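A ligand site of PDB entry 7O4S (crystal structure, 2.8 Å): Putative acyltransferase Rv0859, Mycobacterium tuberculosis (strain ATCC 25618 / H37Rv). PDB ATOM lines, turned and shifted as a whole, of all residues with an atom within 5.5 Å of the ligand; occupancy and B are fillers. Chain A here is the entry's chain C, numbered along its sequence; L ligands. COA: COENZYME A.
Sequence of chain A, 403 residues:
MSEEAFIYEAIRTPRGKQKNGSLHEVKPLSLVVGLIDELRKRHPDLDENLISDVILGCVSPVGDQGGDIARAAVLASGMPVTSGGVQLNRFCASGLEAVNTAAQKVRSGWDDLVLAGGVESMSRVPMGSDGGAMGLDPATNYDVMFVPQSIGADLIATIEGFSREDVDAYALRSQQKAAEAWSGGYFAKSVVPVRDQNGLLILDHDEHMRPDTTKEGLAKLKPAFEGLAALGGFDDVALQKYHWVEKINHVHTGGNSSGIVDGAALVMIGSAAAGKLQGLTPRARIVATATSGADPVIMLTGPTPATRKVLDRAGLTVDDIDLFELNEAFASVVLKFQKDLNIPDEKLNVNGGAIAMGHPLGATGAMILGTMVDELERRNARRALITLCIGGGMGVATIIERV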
ATOM      1  N   GLN A  18      24.521  25.609 -31.995  1.00  0.00           N
ATOM      2  CA  GLN A  18      23.372  24.714 -31.858  1.00  0.00           C
ATOM      3  C   GLN A  18      22.064  25.442 -32.151  1.00  0.00           C
ATOM      4  O   GLN A  18      21.187  24.895 -32.827  1.00  0.00           O
ATOM      5  CB  GLN A  18      23.333  24.119 -30.454  1.00  0.00           C
ATOM      6  CG  GLN A  18      22.088  23.290 -30.163  1.00  0.00           C
ATOM      7  CD  GLN A  18      21.983  22.888 -28.709  1.00  0.00           C
ATOM      8  OE1 GLN A  18      22.501  23.566 -27.823  1.00  0.00           O
ATOM      9  NE2 GLN A  18      21.306  21.771 -28.453  1.00  0.00           N
ATOM     10  N   LYS A  19      21.928  26.663 -31.636  1.00  0.00           N
ATOM     11  CA  LYS A  19      20.718  27.459 -31.824  1.00  0.00           C
ATOM     12  C   LYS A  19      20.994  28.516 -32.882  1.00  0.00           C
ATOM     13  O   LYS A  19      21.935  29.307 -32.742  1.00  0.00           O
ATOM     14  CB  LYS A  19      20.286  28.101 -30.502  1.00  0.00           C
ATOM     15  CG  LYS A  19      20.443  27.172 -29.304  1.00  0.00           C
ATOM     16  CD  LYS A  19      19.580  27.610 -28.126  1.00  0.00           C
ATOM     17  CE  LYS A  19      18.107  27.349 -28.410  1.00  0.00           C
ATOM     18  NZ  LYS A  19      17.241  27.733 -27.262  1.00  0.00           N
ATOM     19  N   CYS A  92      33.789  10.710 -26.720  1.00  0.00           N
ATOM     20  CA  CYS A  92      34.406  11.971 -27.121  1.00  0.00           C
ATOM     21  C   CYS A  92      35.711  11.775 -27.876  1.00  0.00           C
ATOM     22  O   CYS A  92      36.098  12.645 -28.672  1.00  0.00           O
ATOM     23  CB  CYS A  92      34.634  12.842 -25.883  1.00  0.00           C
ATOM     24  SG  CYS A  92      33.132  13.193 -24.942  1.00  0.00           S
ATOM     25  N   MET A 122      25.434  17.971 -34.103  1.00  0.00           N
ATOM     26  CA  MET A 122      24.672  17.883 -32.865  1.00  0.00           C
ATOM     27  C   MET A 122      23.368  18.668 -32.926  1.00  0.00           C
ATOM     28  O   MET A 122      22.451  18.380 -32.149  1.00  0.00           O
ATOM     29  CB  MET A 122      25.518  18.377 -31.689  1.00  0.00           C
ATOM     30  CG  MET A 122      26.832  17.630 -31.530  1.00  0.00           C
ATOM     31  SD  MET A 122      27.703  18.084 -30.016  1.00  0.00           S
ATOM     32  CE  MET A 122      26.620  17.386 -28.778  1.00  0.00           C
ATOM     33  N   MET A 127      22.601  14.817 -28.846  1.00  0.00           N
ATOM     34  CA  MET A 127      23.315  13.862 -28.008  1.00  0.00           C
ATOM     35  C   MET A 127      22.331  12.948 -27.292  1.00  0.00           C
ATOM     36  O   MET A 127      21.389  13.419 -26.639  1.00  0.00           O
ATOM     37  CB  MET A 127      24.182  14.617 -26.995  1.00  0.00           C
ATOM     38  CG  MET A 127      25.163  13.752 -26.223  1.00  0.00           C
ATOM     39  SD  MET A 127      26.173  14.757 -25.124  1.00  0.00           S
ATOM     40  CE  MET A 127      27.282  13.525 -24.447  1.00  0.00           C
ATOM     41  N   GLN A 149      27.952  13.437 -17.528  1.00  0.00           N
ATOM     42  CA  GLN A 149      29.299  13.996 -17.501  1.00  0.00           C
ATOM     43  C   GLN A 149      29.362  15.308 -16.739  1.00  0.00           C
ATOM     44  O   GLN A 149      30.387  15.619 -16.111  1.00  0.00           O
ATOM     45  CB  GLN A 149      29.820  14.200 -18.929  1.00  0.00           C
ATOM     46  CG  GLN A 149      29.912  12.936 -19.748  1.00  0.00           C
ATOM     47  CD  GLN A 149      30.430  13.209 -21.152  1.00  0.00           C
ATOM     48  OE1 GLN A 149      30.463  14.353 -21.595  1.00  0.00           O
ATOM     49  NE2 GLN A 149      30.830  12.152 -21.846  1.00  0.00           N
ATOM     50  N   SER A 150      28.284  16.093 -16.772  1.00  0.00           N
ATOM     51  CA  SER A 150      28.282  17.394 -16.114  1.00  0.00           C
ATOM     52  C   SER A 150      28.445  17.255 -14.602  1.00  0.00           C
ATOM     53  O   SER A 150      29.215  18.004 -13.991  1.00  0.00           O
ATOM     54  CB  SER A 150      26.996  18.133 -16.454  1.00  0.00           C
ATOM     55  OG  SER A 150      25.861  17.334 -16.166  1.00  0.00           O
ATOM     56  N   GLN A 175      38.560  31.659 -24.487  1.00  0.00           N
ATOM     57  CA  GLN A 175      37.966  32.600 -25.427  1.00  0.00           C
ATOM     58  C   GLN A 175      39.012  33.555 -25.997  1.00  0.00           C
ATOM     59  O   GLN A 175      38.989  33.883 -27.190  1.00  0.00           O
ATOM     60  CB  GLN A 175      36.843  33.387 -24.743  1.00  0.00           C
ATOM     61  CG  GLN A 175      35.667  32.540 -24.294  1.00  0.00           C
ATOM     62  CD  GLN A 175      34.725  32.208 -25.432  1.00  0.00           C
ATOM     63  OE1 GLN A 175      34.974  32.554 -26.588  1.00  0.00           O
ATOM     64  NE2 GLN A 175      33.630  31.528 -25.111  1.00  0.00           N
ATOM     65  N   HIS A 208      30.564  29.607 -32.442  1.00  0.00           N
ATOM     66  CA  HIS A 208      30.332  29.535 -31.000  1.00  0.00           C
ATOM     67  C   HIS A 208      31.210  30.516 -30.227  1.00  0.00           C
ATOM     68  O   HIS A 208      30.923  30.783 -29.055  1.00  0.00           O
ATOM     69  CB  HIS A 208      30.560  28.110 -30.497  1.00  0.00           C
ATOM     70  CG  HIS A 208      30.129  27.897 -29.076  1.00  0.00           C
ATOM     71  ND1 HIS A 208      28.814  27.975 -28.681  1.00  0.00           N
ATOM     72  CD2 HIS A 208      30.850  27.606 -27.967  1.00  0.00           C
ATOM     73  CE1 HIS A 208      28.737  27.741 -27.378  1.00  0.00           C
ATOM     74  NE2 HIS A 208      29.963  27.518 -26.918  1.00  0.00           N
ATOM     75  N   ARG A 210      32.847  33.650 -28.500  1.00  0.00           N
ATOM     76  CA  ARG A 210      32.397  34.933 -27.945  1.00  0.00           C
ATOM     77  C   ARG A 210      33.640  35.689 -27.519  1.00  0.00           C
ATOM     78  O   ARG A 210      33.992  35.705 -26.322  1.00  0.00           O
ATOM     79  CB  ARG A 210      31.422  34.731 -26.794  1.00  0.00           C
ATOM     80  CG  ARG A 210      30.252  33.807 -27.135  1.00  0.00           C
ATOM     81  CD  ARG A 210      29.412  33.481 -25.910  1.00  0.00           C
ATOM     82  NE  ARG A 210      28.562  34.601 -25.515  1.00  0.00           N
ATOM     83  CZ  ARG A 210      27.268  34.701 -25.799  1.00  0.00           C
ATOM     84  NH1 ARG A 210      26.664  33.745 -26.490  1.00  0.00           N
ATOM     85  NH2 ARG A 210      26.581  35.770 -25.399  1.00  0.00           N
ATOM     86  N   THR A 213      34.175  38.127 -24.364  1.00  0.00           N
ATOM     87  CA  THR A 213      33.820  37.589 -23.060  1.00  0.00           C
ATOM     88  C   THR A 213      34.598  38.312 -21.959  1.00  0.00           C
ATOM     89  O   THR A 213      35.780  38.617 -22.116  1.00  0.00           O
ATOM     90  CB  THR A 213      34.109  36.085 -23.014  1.00  0.00           C
ATOM     91  OG1 THR A 213      33.312  35.410 -23.993  1.00  0.00           O
ATOM     92  CG2 THR A 213      33.805  35.502 -21.647  1.00  0.00           C
ATOM     93  N   GLY A 217      30.809  38.996 -17.057  1.00  0.00           N
ATOM     94  CA  GLY A 217      29.750  38.328 -17.789  1.00  0.00           C
ATOM     95  C   GLY A 217      29.647  36.858 -17.453  1.00  0.00           C
ATOM     96  O   GLY A 217      28.549  36.303 -17.354  1.00  0.00           O
ATOM     97  N   LEU A 218      30.795  36.190 -17.278  1.00  0.00           N
ATOM     98  CA  LEU A 218      30.789  34.780 -16.904  1.00  0.00           C
ATOM     99  C   LEU A 218      30.225  34.568 -15.514  1.00  0.00           C
ATOM    100  O   LEU A 218      29.644  33.505 -15.233  1.00  0.00           O
ATOM    101  CB  LEU A 218      32.193  34.205 -17.007  1.00  0.00           C
ATOM    102  CG  LEU A 218      32.780  34.081 -18.416  1.00  0.00           C
ATOM    103  CD1 LEU A 218      34.271  33.779 -18.366  1.00  0.00           C
ATOM    104  CD2 LEU A 218      32.044  33.005 -19.200  1.00  0.00           C
ATOM    105  N   LEU A 221      26.265  34.210 -15.253  1.00  0.00           N
ATOM    106  CA  LEU A 221      25.623  33.003 -15.736  1.00  0.00           C
ATOM    107  C   LEU A 221      25.240  32.097 -14.571  1.00  0.00           C
ATOM    108  O   LEU A 221      25.857  32.107 -13.504  1.00  0.00           O
ATOM    109  CB  LEU A 221      26.547  32.254 -16.698  1.00  0.00           C
ATOM    110  CG  LEU A 221      27.073  33.074 -17.872  1.00  0.00           C
ATOM    111  CD1 LEU A 221      27.856  32.207 -18.832  1.00  0.00           C
ATOM    112  CD2 LEU A 221      25.932  33.785 -18.593  1.00  0.00           C
ATOM    113  N   ALA A 224      24.176  25.517 -15.084  1.00  0.00           N
ATOM    114  CA  ALA A 224      23.308  24.883 -16.066  1.00  0.00           C
ATOM    115  C   ALA A 224      22.892  23.477 -15.668  1.00  0.00           C
ATOM    116  O   ALA A 224      21.838  22.994 -16.103  1.00  0.00           O
ATOM    117  CB  ALA A 224      23.999  24.850 -17.436  1.00  0.00           C
ATOM    118  N   PHE A 225      23.693  22.800 -14.844  1.00  0.00           N
ATOM    119  CA  PHE A 225      23.473  21.397 -14.526  1.00  0.00           C
ATOM    120  C   PHE A 225      22.981  21.186 -13.098  1.00  0.00           C
ATOM    121  O   PHE A 225      23.025  20.065 -12.589  1.00  0.00           O
ATOM    122  CB  PHE A 225      24.750  20.598 -14.769  1.00  0.00           C
ATOM    123  CG  PHE A 225      25.444  20.960 -16.056  1.00  0.00           C
ATOM    124  CD1 PHE A 225      24.864  20.680 -17.276  1.00  0.00           C
ATOM    125  CD2 PHE A 225      26.682  21.577 -16.027  1.00  0.00           C
ATOM    126  CE1 PHE A 225      25.501  21.018 -18.458  1.00  0.00           C
ATOM    127  CE2 PHE A 225      27.328  21.910 -17.200  1.00  0.00           C
ATOM    128  CZ  PHE A 225      26.737  21.629 -18.411  1.00  0.00           C
ATOM    129  N   THR A 253      28.762  26.406 -16.028  1.00  0.00           N
ATOM    130  CA  THR A 253      27.672  27.075 -16.727  1.00  0.00           C
ATOM    131  C   THR A 253      27.875  26.895 -18.237  1.00  0.00           C
ATOM    132  O   THR A 253      28.757  26.168 -18.686  1.00  0.00           O
ATOM    133  CB  THR A 253      27.618  28.555 -16.351  1.00  0.00           C
ATOM    134  OG1 THR A 253      28.723  29.240 -16.935  1.00  0.00           O
ATOM    135  CG2 THR A 253      27.668  28.713 -14.830  1.00  0.00           C
ATOM    136  N   GLY A 254      27.035  27.577 -19.019  1.00  0.00           N
ATOM    137  CA  GLY A 254      27.196  27.568 -20.462  1.00  0.00           C
ATOM    138  C   GLY A 254      28.396  28.343 -20.965  1.00  0.00           C
ATOM    139  O   GLY A 254      28.699  28.273 -22.154  1.00  0.00           O
ATOM    140  N   GLY A 255      29.080  29.069 -20.083  1.00  0.00           N
ATOM    141  CA  GLY A 255      30.224  29.865 -20.487  1.00  0.00           C
ATOM    142  C   GLY A 255      31.552  29.220 -20.196  1.00  0.00           C
ATOM    143  O   GLY A 255      32.581  29.627 -20.743  1.00  0.00           O
ATOM    144  N   SER A 257      31.650  25.585 -20.069  1.00  0.00           N
ATOM    145  CA  SER A 257      31.516  24.224 -20.557  1.00  0.00           C
ATOM    146  C   SER A 257      31.657  24.215 -22.076  1.00  0.00           C
ATOM    147  O   SER A 257      31.526  25.239 -22.741  1.00  0.00           O
ATOM    148  CB  SER A 257      30.164  23.630 -20.151  1.00  0.00           C
ATOM    149  OG  SER A 257      30.010  23.628 -18.743  1.00  0.00           O
ATOM    150  N   SER A 258      31.923  23.025 -22.612  1.00  0.00           N
ATOM    151  CA  SER A 258      32.084  22.883 -24.048  1.00  0.00           C
ATOM    152  C   SER A 258      30.768  23.206 -24.756  1.00  0.00           C
ATOM    153  O   SER A 258      29.680  22.941 -24.260  1.00  0.00           O
ATOM    154  CB  SER A 258      32.533  21.461 -24.397  1.00  0.00           C
ATOM    155  OG  SER A 258      31.586  20.500 -23.970  1.00  0.00           O
ATOM    156  N   GLY A 259      30.898  23.789 -25.945  1.00  0.00           N
ATOM    157  CA  GLY A 259      29.723  24.145 -26.716  1.00  0.00           C
ATOM    158  C   GLY A 259      29.214  22.989 -27.553  1.00  0.00           C
ATOM    159  O   GLY A 259      29.966  22.154 -28.038  1.00  0.00           O
ATOM    160  N   ILE A 260      27.888  22.955 -27.717  1.00  0.00           N
ATOM    161  CA  ILE A 260      27.228  21.985 -28.575  1.00  0.00           C
ATOM    162  C   ILE A 260      27.182  22.569 -29.979  1.00  0.00           C
ATOM    163  O   ILE A 260      26.441  23.521 -30.248  1.00  0.00           O
ATOM    164  CB  ILE A 260      25.825  21.649 -28.064  1.00  0.00           C
ATOM    165  CG1 ILE A 260      25.909  20.969 -26.690  1.00  0.00           C
ATOM    166  CG2 ILE A 260      25.083  20.770 -29.056  1.00  0.00           C
ATOM    167  CD1 ILE A 260      24.555  20.701 -26.067  1.00  0.00           C
ATOM    168  N   ALA A 329      36.164  19.901 -22.542  1.00  0.00           N
ATOM    169  CA  ALA A 329      34.796  19.464 -22.285  1.00  0.00           C
ATOM    170  C   ALA A 329      34.189  20.241 -21.131  1.00  0.00           C
ATOM    171  O   ALA A 329      33.066  20.751 -21.219  1.00  0.00           O
ATOM    172  CB  ALA A 329      34.768  17.960 -21.998  1.00  0.00           C
ATOM    173  N   PHE A 330      34.933  20.350 -20.031  1.00  0.00           N
ATOM    174  CA  PHE A 330      34.578  21.194 -18.899  1.00  0.00           C
ATOM    175  C   PHE A 330      35.847  21.795 -18.333  1.00  0.00           C
ATOM    176  O   PHE A 330      36.929  21.209 -18.433  1.00  0.00           O
ATOM    177  CB  PHE A 330      33.822  20.408 -17.815  1.00  0.00           C
ATOM    178  CG  PHE A 330      32.505  19.859 -18.282  1.00  0.00           C
ATOM    179  CD1 PHE A 330      31.334  20.592 -18.139  1.00  0.00           C
ATOM    180  CD2 PHE A 330      32.426  18.603 -18.857  1.00  0.00           C
ATOM    181  CE1 PHE A 330      30.119  20.080 -18.564  1.00  0.00           C
ATOM    182  CE2 PHE A 330      31.221  18.092 -19.291  1.00  0.00           C
ATOM    183  CZ  PHE A 330      30.062  18.832 -19.145  1.00  0.00           C
ATOM    184  N   HIS A 359      32.431  21.624 -29.372  1.00  0.00           N
ATOM    185  CA  HIS A 359      32.817  20.225 -29.166  1.00  0.00           C
ATOM    186  C   HIS A 359      31.908  19.331 -30.007  1.00  0.00           C
ATOM    187  O   HIS A 359      30.940  18.748 -29.495  1.00  0.00           O
ATOM    188  CB  HIS A 359      32.742  19.861 -27.686  1.00  0.00           C
ATOM    189  CG  HIS A 359      33.135  18.445 -27.379  1.00  0.00           C
ATOM    190  ND1 HIS A 359      33.733  17.617 -28.297  1.00  0.00           N
ATOM    191  CD2 HIS A 359      33.011  17.715 -26.240  1.00  0.00           C
ATOM    192  CE1 HIS A 359      33.968  16.433 -27.742  1.00  0.00           C
ATOM    193  NE2 HIS A 359      33.535  16.478 -26.487  1.00  0.00           N
ATOM    194  N   LEU A 361      31.186  16.081 -30.942  1.00  0.00           N
ATOM    195  CA  LEU A 361      31.627  14.853 -30.282  1.00  0.00           C
ATOM    196  C   LEU A 361      32.519  13.967 -31.144  1.00  0.00           C
ATOM    197  O   LEU A 361      33.688  13.731 -30.821  1.00  0.00           O
ATOM    198  CB  LEU A 361      30.394  14.071 -29.826  1.00  0.00           C
ATOM    199  CG  LEU A 361      29.353  14.804 -28.984  1.00  0.00           C
ATOM    200  CD1 LEU A 361      28.302  13.834 -28.462  1.00  0.00           C
ATOM    201  CD2 LEU A 361      30.006  15.565 -27.847  1.00  0.00           C
HETATM  202  N1A COA L   1      29.890  34.970 -22.110  1.00  0.00           N
HETATM  203  C2A COA L   1      28.683  35.459 -21.809  1.00  0.00           C
HETATM  204  N3A COA L   1      27.499  34.851 -21.809  1.00  0.00           N
HETATM  205  C4A COA L   1      27.641  33.564 -22.176  1.00  0.00           C
HETATM  206  C5A COA L   1      28.809  32.916 -22.524  1.00  0.00           C
HETATM  207  C6A COA L   1      29.997  33.669 -22.474  1.00  0.00           C
HETATM  208  N6A COA L   1      31.196  33.185 -22.784  1.00  0.00           N
HETATM  209  N7A COA L   1      28.542  31.594 -22.849  1.00  0.00           N
HETATM  210  C8A COA L   1      27.237  31.465 -22.704  1.00  0.00           C
HETATM  211  N9A COA L   1      26.637  32.639 -22.293  1.00  0.00           N
HETATM  212  C1B COA L   1      25.224  32.869 -22.044  1.00  0.00           C
HETATM  213  C2B COA L   1      24.348  32.689 -23.283  1.00  0.00           C
HETATM  214  O2B COA L   1      24.257  33.839 -24.083  1.00  0.00           O
HETATM  215  C3B COA L   1      23.030  32.272 -22.634  1.00  0.00           C
HETATM  216  O3B COA L   1      22.446  33.423 -22.018  1.00  0.00           O
HETATM  217  P3B COA L   1      20.838  33.364 -22.137  1.00  0.00           P
HETATM  218  O7A COA L   1      20.520  33.243 -23.611  1.00  0.00           O
HETATM  219  O8A COA L   1      20.371  32.162 -21.333  1.00  0.00           O
HETATM  220  O9A COA L   1      20.332  34.669 -21.546  1.00  0.00           O
HETATM  221  C4B COA L   1      23.546  31.299 -21.584  1.00  0.00           C
HETATM  222  O4B COA L   1      24.752  31.942 -21.093  1.00  0.00           O
HETATM  223  C5B COA L   1      23.939  29.952 -22.133  1.00  0.00           C
HETATM  224  O5B COA L   1      23.226  29.720 -23.368  1.00  0.00           O
HETATM  225  P1A COA L   1      23.920  28.785 -24.475  1.00  0.00           P
HETATM  226  O1A COA L   1      25.355  29.159 -24.600  1.00  0.00           O
HETATM  227  O2A COA L   1      23.089  28.789 -25.711  1.00  0.00           O
HETATM  228  O3A COA L   1      23.824  27.334 -23.803  1.00  0.00           O
HETATM  229  P2A COA L   1      22.591  26.418 -23.340  1.00  0.00           P
HETATM  230  O4A COA L   1      21.915  27.038 -22.160  1.00  0.00           O
HETATM  231  O5A COA L   1      21.768  26.069 -24.539  1.00  0.00           O
HETATM  232  O6A COA L   1      23.379  25.097 -22.866  1.00  0.00           O
HETATM  233  CBP COA L   1      25.100  23.875 -21.694  1.00  0.00           C
HETATM  234  CCP COA L   1      24.605  25.256 -22.105  1.00  0.00           C
HETATM  235  CDP COA L   1      26.377  24.028 -20.858  1.00  0.00           C
HETATM  236  CEP COA L   1      24.023  23.212 -20.826  1.00  0.00           C
HETATM  237  CAP COA L   1      25.404  22.990 -22.919  1.00  0.00           C
HETATM  238  OAP COA L   1      26.251  23.722 -23.792  1.00  0.00           O
HETATM  239  C9P COA L   1      26.070  21.680 -22.545  1.00  0.00           C
HETATM  240  O9P COA L   1      25.422  20.801 -21.973  1.00  0.00           O
HETATM  241  N8P COA L   1      27.348  21.529 -22.862  1.00  0.00           N
HETATM  242  C7P COA L   1      28.207  20.545 -22.224  1.00  0.00           C
HETATM  243  C6P COA L   1      28.565  19.405 -23.140  1.00  0.00           C
HETATM  244  C5P COA L   1      28.058  18.086 -22.591  1.00  0.00           C
HETATM  245  O5P COA L   1      27.389  18.051 -21.562  1.00  0.00           O
HETATM  246  N4P COA L   1      28.375  16.981 -23.276  1.00  0.00           N
HETATM  247  C3P COA L   1      29.227  16.972 -24.455  1.00  0.00           C
HETATM  248  C2P COA L   1      30.403  16.034 -24.308  1.00  0.00           C
HETATM  249  S1P COA L   1      31.475  16.474 -22.922  1.00  0.00           S
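O of Ala 329 lies within hydrogen-bond range of N of Ser 258 (2.9 Å). The backbone carbonyl oxygen of Arg 210 lies within hydrogen-bond range of the side-chain hydroxyl of Thr 213 (2.4 Å). N of Arg 210 sits at hydrogen-bond distance from OE1 of Gln 175 (3.1 Å). The backbone NH of Gly 255 sits close to the side-chain hydroxyl of Thr 253 (3.2 Å). The side-chain sulfur of Cys 92 is in hydrogen-bond range of a ring nitrogen (NE2) of His 359 (3.7 Å). The backbone carbonyl oxygen (O) of Gly 259 is in hydrogen-bond range of the backbone NH (N) of His 359, at 2.9 Å. The backbone carbonyl oxygen of Thr 253 lies within hydrogen-bond range of the side-chain hydroxyl of Ser 257 (2.8 Å). The backbone NH (N) of Gln 18 sits close to the backbone carbonyl oxygen (O) of Ile 260 (3.3 Å).
S1P of the ligand sits close to OE1 of Gln 149 (2.7 Å). O of Ser 258 is in hydrogen-bond range of N8P of the ligand, 3.1 Å away. O2B of the ligand is in hydrogen-bond range of NH2 of Arg 210, 3.3 Å away. The side-chain hydroxyl (OG1) of Thr 213 is in hydrogen-bond range of a nitrogen (N6A) of the ligand (3.3 Å). A nitrogen (N4P) of the ligand is in hydrogen-bond range of the side-chain sulfur of Met 127 (3.6 Å).
The backbone carbonyl oxygen (O) of Gly 254 sits close to a nitrogen (N7A) of the ligand (3.4 Å). SG of Cys 92 touches C2P of the ligand, at 3.99 Å. NE2 of Gln 175 touches N6A of the ligand, 3.8 Å away. Leu 218 touches the ligand. Leu 221 touches the ligand (CD2 to O4B, 3.3 Å). Ala 224 touches the ligand. Phe 225 touches the ligand (CZ to CDP, 3.4 Å). Thr 253 touches the ligand. Gly 255 touches the ligand. Ser 257 touches the ligand. Ile 260 touches the ligand (CD1 to C9P, 3.96 Å). CB of Ala 329 touches S1P of the ligand (3.7 Å). CZ of Phe 330 touches O5P of the ligand, 3.7 Å away. CD2 of His 359 touches C2P of the ligand (3.7 Å). CD2 of Leu 361 touches C2P of the ligand, 3.6 Å away. Hydrophobic or aromatic side chains that line the ligand: Met 127, Leu 218, Leu 221, Ala 224, Phe 225, Ile 260, Ala 329, Phe 330, His 359 and Leu 361. 20 residues have an atom within 4 Å of the ligand: Cys 92, Met 127, Gln 149, Gln 175, Arg 210, Thr 213, Leu 218, Leu 221, Ala 224, Phe 225, Thr 253, Gly 254, Gly 255, Ser 257, Ser 258, Ile 260, Ala 329, Phe 330, His 359 and Leu 361.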
